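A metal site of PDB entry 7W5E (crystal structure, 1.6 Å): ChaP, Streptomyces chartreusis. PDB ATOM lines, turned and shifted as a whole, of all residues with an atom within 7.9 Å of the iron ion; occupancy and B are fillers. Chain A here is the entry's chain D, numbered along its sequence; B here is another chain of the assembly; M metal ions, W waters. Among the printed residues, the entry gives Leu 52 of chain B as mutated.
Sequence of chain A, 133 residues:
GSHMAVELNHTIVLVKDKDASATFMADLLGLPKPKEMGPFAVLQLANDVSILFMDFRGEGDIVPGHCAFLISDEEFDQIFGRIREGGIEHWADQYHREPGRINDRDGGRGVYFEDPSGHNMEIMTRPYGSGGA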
ATOM      1  N   PRO A  64      -5.496  30.111  17.393  1.00  0.00           N
ATOM      2  CA  PRO A  64      -4.737  28.867  17.590  1.00  0.00           C
ATOM      3  C   PRO A  64      -4.867  27.857  16.455  1.00  0.00           C
ATOM      4  O   PRO A  64      -4.633  26.672  16.707  1.00  0.00           O
ATOM      5  CB  PRO A  64      -5.338  28.306  18.871  1.00  0.00           C
ATOM      6  CG  PRO A  64      -6.758  28.752  18.839  1.00  0.00           C
ATOM      7  CD  PRO A  64      -6.800  30.061  18.085  1.00  0.00           C
ATOM      8  N   GLY A  65      -5.263  28.301  15.259  1.00  0.00           N
ATOM      9  CA  GLY A  65      -5.289  27.390  14.130  1.00  0.00           C
ATOM     10  C   GLY A  65      -3.918  26.813  13.833  1.00  0.00           C
ATOM     11  O   GLY A  65      -2.896  27.446  14.079  1.00  0.00           O
ATOM     12  N   HIS A  66      -3.915  25.584  13.335  1.00  0.00           N
ATOM     13  CA  HIS A  66      -2.670  24.924  12.944  1.00  0.00           C
ATOM     14  C   HIS A  66      -2.999  23.656  12.154  1.00  0.00           C
ATOM     15  O   HIS A  66      -4.142  23.198  12.144  1.00  0.00           O
ATOM     16  CB  HIS A  66      -1.784  24.581  14.143  1.00  0.00           C
ATOM     17  CG  HIS A  66      -2.469  23.774  15.212  1.00  0.00           C
ATOM     18  ND1 HIS A  66      -3.388  24.312  16.087  1.00  0.00           N
ATOM     19  CD2 HIS A  66      -2.355  22.462  15.545  1.00  0.00           C
ATOM     20  CE1 HIS A  66      -3.797  23.364  16.921  1.00  0.00           C
ATOM     21  NE2 HIS A  66      -3.184  22.238  16.612  1.00  0.00           N
ATOM     22  N   CYS A  67      -1.981  23.126  11.496  1.00  0.00           N
ATOM     23  CA  CYS A  67      -1.991  21.776  10.943  1.00  0.00           C
ATOM     24  C   CYS A  67      -1.018  20.920  11.736  1.00  0.00           C
ATOM     25  O   CYS A  67       0.143  21.314  11.931  1.00  0.00           O
ATOM     26  CB  CYS A  67      -1.598  21.765   9.468  1.00  0.00           C
ATOM     27  SG  CYS A  67      -2.785  22.494   8.329  1.00  0.00           S
ATOM     28  N   ALA A  68      -1.461  19.749  12.182  1.00  0.00           N
ATOM     29  CA  ALA A  68      -0.694  18.920  13.100  1.00  0.00           C
ATOM     30  C   ALA A  68      -0.373  17.580  12.472  1.00  0.00           C
ATOM     31  O   ALA A  68      -1.222  16.944  11.841  1.00  0.00           O
ATOM     32  CB  ALA A  68      -1.445  18.701  14.393  1.00  0.00           C
ATOM     33  N   PHE A  69       0.880  17.148  12.660  1.00  0.00           N
ATOM     34  CA  PHE A  69       1.390  15.908  12.102  1.00  0.00           C
ATOM     35  C   PHE A  69       1.769  14.963  13.233  1.00  0.00           C
ATOM     36  O   PHE A  69       2.445  15.359  14.182  1.00  0.00           O
ATOM     37  CB  PHE A  69       2.576  16.175  11.177  1.00  0.00           C
ATOM     38  CG  PHE A  69       2.259  17.133  10.060  1.00  0.00           C
ATOM     39  CD1 PHE A  69       2.378  18.487  10.256  1.00  0.00           C
ATOM     40  CD2 PHE A  69       1.778  16.656   8.849  1.00  0.00           C
ATOM     41  CE1 PHE A  69       2.056  19.374   9.242  1.00  0.00           C
ATOM     42  CE2 PHE A  69       1.448  17.538   7.834  1.00  0.00           C
ATOM     43  CZ  PHE A  69       1.590  18.893   8.031  1.00  0.00           C
ATOM     44  N   GLN A  94      -0.559  25.913  21.343  1.00  0.00           N
ATOM     45  CA  GLN A  94      -1.182  26.352  20.095  1.00  0.00           C
ATOM     46  C   GLN A  94      -1.391  27.865  20.042  1.00  0.00           C
ATOM     47  O   GLN A  94      -1.643  28.401  18.953  1.00  0.00           O
ATOM     48  CB  GLN A  94      -2.512  25.616  19.905  1.00  0.00           C
ATOM     49  CG  GLN A  94      -3.490  25.836  21.045  1.00  0.00           C
ATOM     50  CD  GLN A  94      -4.777  25.069  20.854  1.00  0.00           C
ATOM     51  OE1 GLN A  94      -4.989  24.449  19.809  1.00  0.00           O
ATOM     52  NE2 GLN A  94      -5.636  25.079  21.865  1.00  0.00           N
ATOM     53  N   TYR A 112       4.880  23.359  18.639  1.00  0.00           N
ATOM     54  CA  TYR A 112       4.278  24.170  17.605  1.00  0.00           C
ATOM     55  C   TYR A 112       5.323  25.112  17.009  1.00  0.00           C
ATOM     56  O   TYR A 112       6.279  25.504  17.689  1.00  0.00           O
ATOM     57  CB  TYR A 112       3.101  25.000  18.149  1.00  0.00           C
ATOM     58  CG  TYR A 112       1.999  24.183  18.785  1.00  0.00           C
ATOM     59  CD1 TYR A 112       2.150  23.662  20.074  1.00  0.00           C
ATOM     60  CD2 TYR A 112       0.824  23.938  18.113  1.00  0.00           C
ATOM     61  CE1 TYR A 112       1.138  22.917  20.662  1.00  0.00           C
ATOM     62  CE2 TYR A 112      -0.190  23.182  18.680  1.00  0.00           C
ATOM     63  CZ  TYR A 112      -0.027  22.681  19.961  1.00  0.00           C
ATOM     64  OH  TYR A 112      -1.043  21.947  20.530  1.00  0.00           O
ATOM     65  N   MET A 121       2.077  25.270  12.444  1.00  0.00           N
ATOM     66  CA  MET A 121       2.223  23.820  12.401  1.00  0.00           C
ATOM     67  C   MET A 121       2.334  23.264  13.814  1.00  0.00           C
ATOM     68  O   MET A 121       2.569  23.975  14.789  1.00  0.00           O
ATOM     69  CB  MET A 121       3.456  23.412  11.583  1.00  0.00           C
ATOM     70  CG  MET A 121       3.542  24.098  10.223  1.00  0.00           C
ATOM     71  SD  MET A 121       2.249  23.572   9.081  1.00  0.00           S
ATOM     72  CE  MET A 121       2.886  24.236   7.541  1.00  0.00           C
ATOM     73  N   GLU A 122       2.180  21.935  13.902  1.00  0.00           N
ATOM     74  CA  GLU A 122       2.385  21.182  15.127  1.00  0.00           C
ATOM     75  C   GLU A 122       2.937  19.823  14.738  1.00  0.00           C
ATOM     76  O   GLU A 122       2.507  19.265  13.731  1.00  0.00           O
ATOM     77  CB  GLU A 122       1.085  21.007  15.927  1.00  0.00           C
ATOM     78  CG  GLU A 122       1.251  20.279  17.263  1.00  0.00           C
ATOM     79  CD  GLU A 122      -0.084  19.887  17.876  1.00  0.00           C
ATOM     80  OE1 GLU A 122      -1.127  20.255  17.318  1.00  0.00           O
ATOM     81  OE2 GLU A 122      -0.075  19.214  18.940  1.00  0.00           O
ATOM     82  N   ILE A 123       3.901  19.317  15.500  1.00  0.00           N
ATOM     83  CA  ILE A 123       4.291  17.915  15.432  1.00  0.00           C
ATOM     84  C   ILE A 123       4.054  17.300  16.804  1.00  0.00           C
ATOM     85  O   ILE A 123       4.246  17.957  17.832  1.00  0.00           O
ATOM     86  CB  ILE A 123       5.751  17.723  14.981  1.00  0.00           C
ATOM     87  CG1 ILE A 123       6.715  18.527  15.867  1.00  0.00           C
ATOM     88  CG2 ILE A 123       5.904  18.105  13.519  1.00  0.00           C
ATOM     89  CD1 ILE A 123       8.188  18.221  15.606  1.00  0.00           C
ATOM     90  N   MET A 124       3.619  16.041  16.817  1.00  0.00           N
ATOM     91  CA  MET A 124       3.211  15.367  18.043  1.00  0.00           C
ATOM     92  C   MET A 124       3.548  13.891  17.905  1.00  0.00           C
ATOM     93  O   MET A 124       3.629  13.362  16.792  1.00  0.00           O
ATOM     94  CB  MET A 124       1.704  15.534  18.308  1.00  0.00           C
ATOM     95  CG  MET A 124       0.838  15.060  17.161  1.00  0.00           C
ATOM     96  SD  MET A 124      -0.912  15.449  17.349  1.00  0.00           S
ATOM     97  CE  MET A 124      -1.513  13.943  18.092  1.00  0.00           C
ATOM     98  N   ASN B   9      -2.500  14.474  11.371  1.00  0.00           N
ATOM     99  CA  ASN B   9      -3.372  14.044  12.464  1.00  0.00           C
ATOM    100  C   ASN B   9      -4.593  14.937  12.640  1.00  0.00           C
ATOM    101  O   ASN B   9      -5.680  14.429  12.939  1.00  0.00           O
ATOM    102  CB  ASN B   9      -2.577  13.990  13.761  1.00  0.00           C
ATOM    103  CG  ASN B   9      -3.392  13.438  14.913  1.00  0.00           C
ATOM    104  OD1 ASN B   9      -3.973  14.193  15.686  1.00  0.00           O
ATOM    105  ND2 ASN B   9      -3.436  12.117  15.027  1.00  0.00           N
ATOM    106  N   HIS B  10      -4.440  16.256  12.511  1.00  0.00           N
ATOM    107  CA  HIS B  10      -5.615  17.117  12.555  1.00  0.00           C
ATOM    108  C   HIS B  10      -5.270  18.476  11.955  1.00  0.00           C
ATOM    109  O   HIS B  10      -4.105  18.832  11.794  1.00  0.00           O
ATOM    110  CB  HIS B  10      -6.184  17.271  13.977  1.00  0.00           C
ATOM    111  CG  HIS B  10      -5.211  17.787  14.993  1.00  0.00           C
ATOM    112  ND1 HIS B  10      -4.320  16.973  15.657  1.00  0.00           N
ATOM    113  CD2 HIS B  10      -5.042  19.039  15.502  1.00  0.00           C
ATOM    114  CE1 HIS B  10      -3.622  17.698  16.513  1.00  0.00           C
ATOM    115  NE2 HIS B  10      -4.046  18.950  16.442  1.00  0.00           N
ATOM    116  N   THR B  11      -6.326  19.200  11.566  1.00  0.00           N
ATOM    117  CA  THR B  11      -6.187  20.555  11.047  1.00  0.00           C
ATOM    118  C   THR B  11      -7.380  21.370  11.509  1.00  0.00           C
ATOM    119  O   THR B  11      -8.482  20.853  11.665  1.00  0.00           O
ATOM    120  CB  THR B  11      -6.072  20.589   9.515  1.00  0.00           C
ATOM    121  OG1 THR B  11      -5.807  21.931   9.092  1.00  0.00           O
ATOM    122  CG2 THR B  11      -7.358  20.098   8.851  1.00  0.00           C
ATOM    123  N   ILE B  12      -7.119  22.652  11.773  1.00  0.00           N
ATOM    124  CA  ILE B  12      -8.126  23.580  12.265  1.00  0.00           C
ATOM    125  C   ILE B  12      -8.693  24.342  11.075  1.00  0.00           C
ATOM    126  O   ILE B  12      -7.942  24.863  10.250  1.00  0.00           O
ATOM    127  CB  ILE B  12      -7.534  24.541  13.313  1.00  0.00           C
ATOM    128  CG1 ILE B  12      -7.393  23.865  14.685  1.00  0.00           C
ATOM    129  CG2 ILE B  12      -8.420  25.795  13.474  1.00  0.00           C
ATOM    130  CD1 ILE B  12      -6.446  22.665  14.744  1.00  0.00           C
ATOM    131  N   PHE B  40     -12.841  24.591  19.865  1.00  0.00           N
ATOM    132  CA  PHE B  40     -13.088  23.846  18.643  1.00  0.00           C
ATOM    133  C   PHE B  40     -14.298  22.936  18.752  1.00  0.00           C
ATOM    134  O   PHE B  40     -14.662  22.468  19.832  1.00  0.00           O
ATOM    135  CB  PHE B  40     -11.860  22.998  18.271  1.00  0.00           C
ATOM    136  CG  PHE B  40     -10.586  23.779  18.191  1.00  0.00           C
ATOM    137  CD1 PHE B  40     -10.456  24.831  17.286  1.00  0.00           C
ATOM    138  CD2 PHE B  40      -9.501  23.451  18.998  1.00  0.00           C
ATOM    139  CE1 PHE B  40      -9.276  25.554  17.206  1.00  0.00           C
ATOM    140  CE2 PHE B  40      -8.315  24.167  18.907  1.00  0.00           C
ATOM    141  CZ  PHE B  40      -8.199  25.221  18.012  1.00  0.00           C
ATOM    142  N   LEU B  52     -10.961  20.265  13.073  1.00  0.00           N
ATOM    143  CA  LEU B  52     -11.310  21.071  14.235  1.00  0.00           C
ATOM    144  C   LEU B  52     -11.860  22.410  13.755  1.00  0.00           C
ATOM    145  O   LEU B  52     -11.096  23.284  13.311  1.00  0.00           O
ATOM    146  CB  LEU B  52     -10.088  21.255  15.144  1.00  0.00           C
ATOM    147  CG  LEU B  52      -9.773  20.096  16.107  1.00  0.00           C
ATOM    148  CD1 LEU B  52      -9.232  18.878  15.371  1.00  0.00           C
ATOM    149  CD2 LEU B  52      -8.779  20.551  17.158  1.00  0.00           C
HETATM  150 FE    FE M   1      -3.113  20.401  17.670  1.00  0.00          FE
HETATM  151  O   HOH W   1      -2.468  18.760  19.370  1.00  0.00           O
HETATM  152  O   HOH W   2      -5.185  20.726  18.774  1.00  0.00           O
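Merely in contact with the iron ion: Tyr 112. Four residues have an atom within 4 Å of the iron ion: His 66, Tyr 112, Glu 122 and His 10 of chain B. Along chain A the residues within 4 Å of the iron ion span positions 66 to 122. The nearest printed residue that does not touch the iron ion is Ala 68 (4.1 Å).
The iron ion is bound by the side-chain carboxylate (OE1) of Glu 122 (2.0 Å). NE2 of His 10 of chain B binds the iron ion (2.1 Å). NE2 of His 66 is bound to the iron ion, at 2.1 Å. Water W2 is bound to the iron ion, 2.4 Å away. Water W1 binds the iron ion, 2.4 Å away.
OH of Tyr 112 is in hydrogen-bond range of OE2 of Glu 122 (3.3 Å). The backbone NH of Glu 122 sits at hydrogen-bond distance from the backbone carbonyl oxygen of Cys 67 (2.9 Å). O of Glu 122 is in hydrogen-bond range of N of Phe 69 (2.9 Å). N of Ala 68 is in hydrogen-bond range of O of His 10 of chain B, at 2.8 Å. A ring nitrogen (ND1) of His 10 of chain B is in hydrogen-bond range of the side-chain amide oxygen of Asn 9 of chain B, at 2.8 Å. O of His 66 lies within hydrogen-bond range of N of Ile 12 of chain B (3.0 Å). A ring nitrogen (ND1) of His 66 lies within hydrogen-bond range of the backbone carbonyl oxygen of Pro 64 (2.7 Å).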
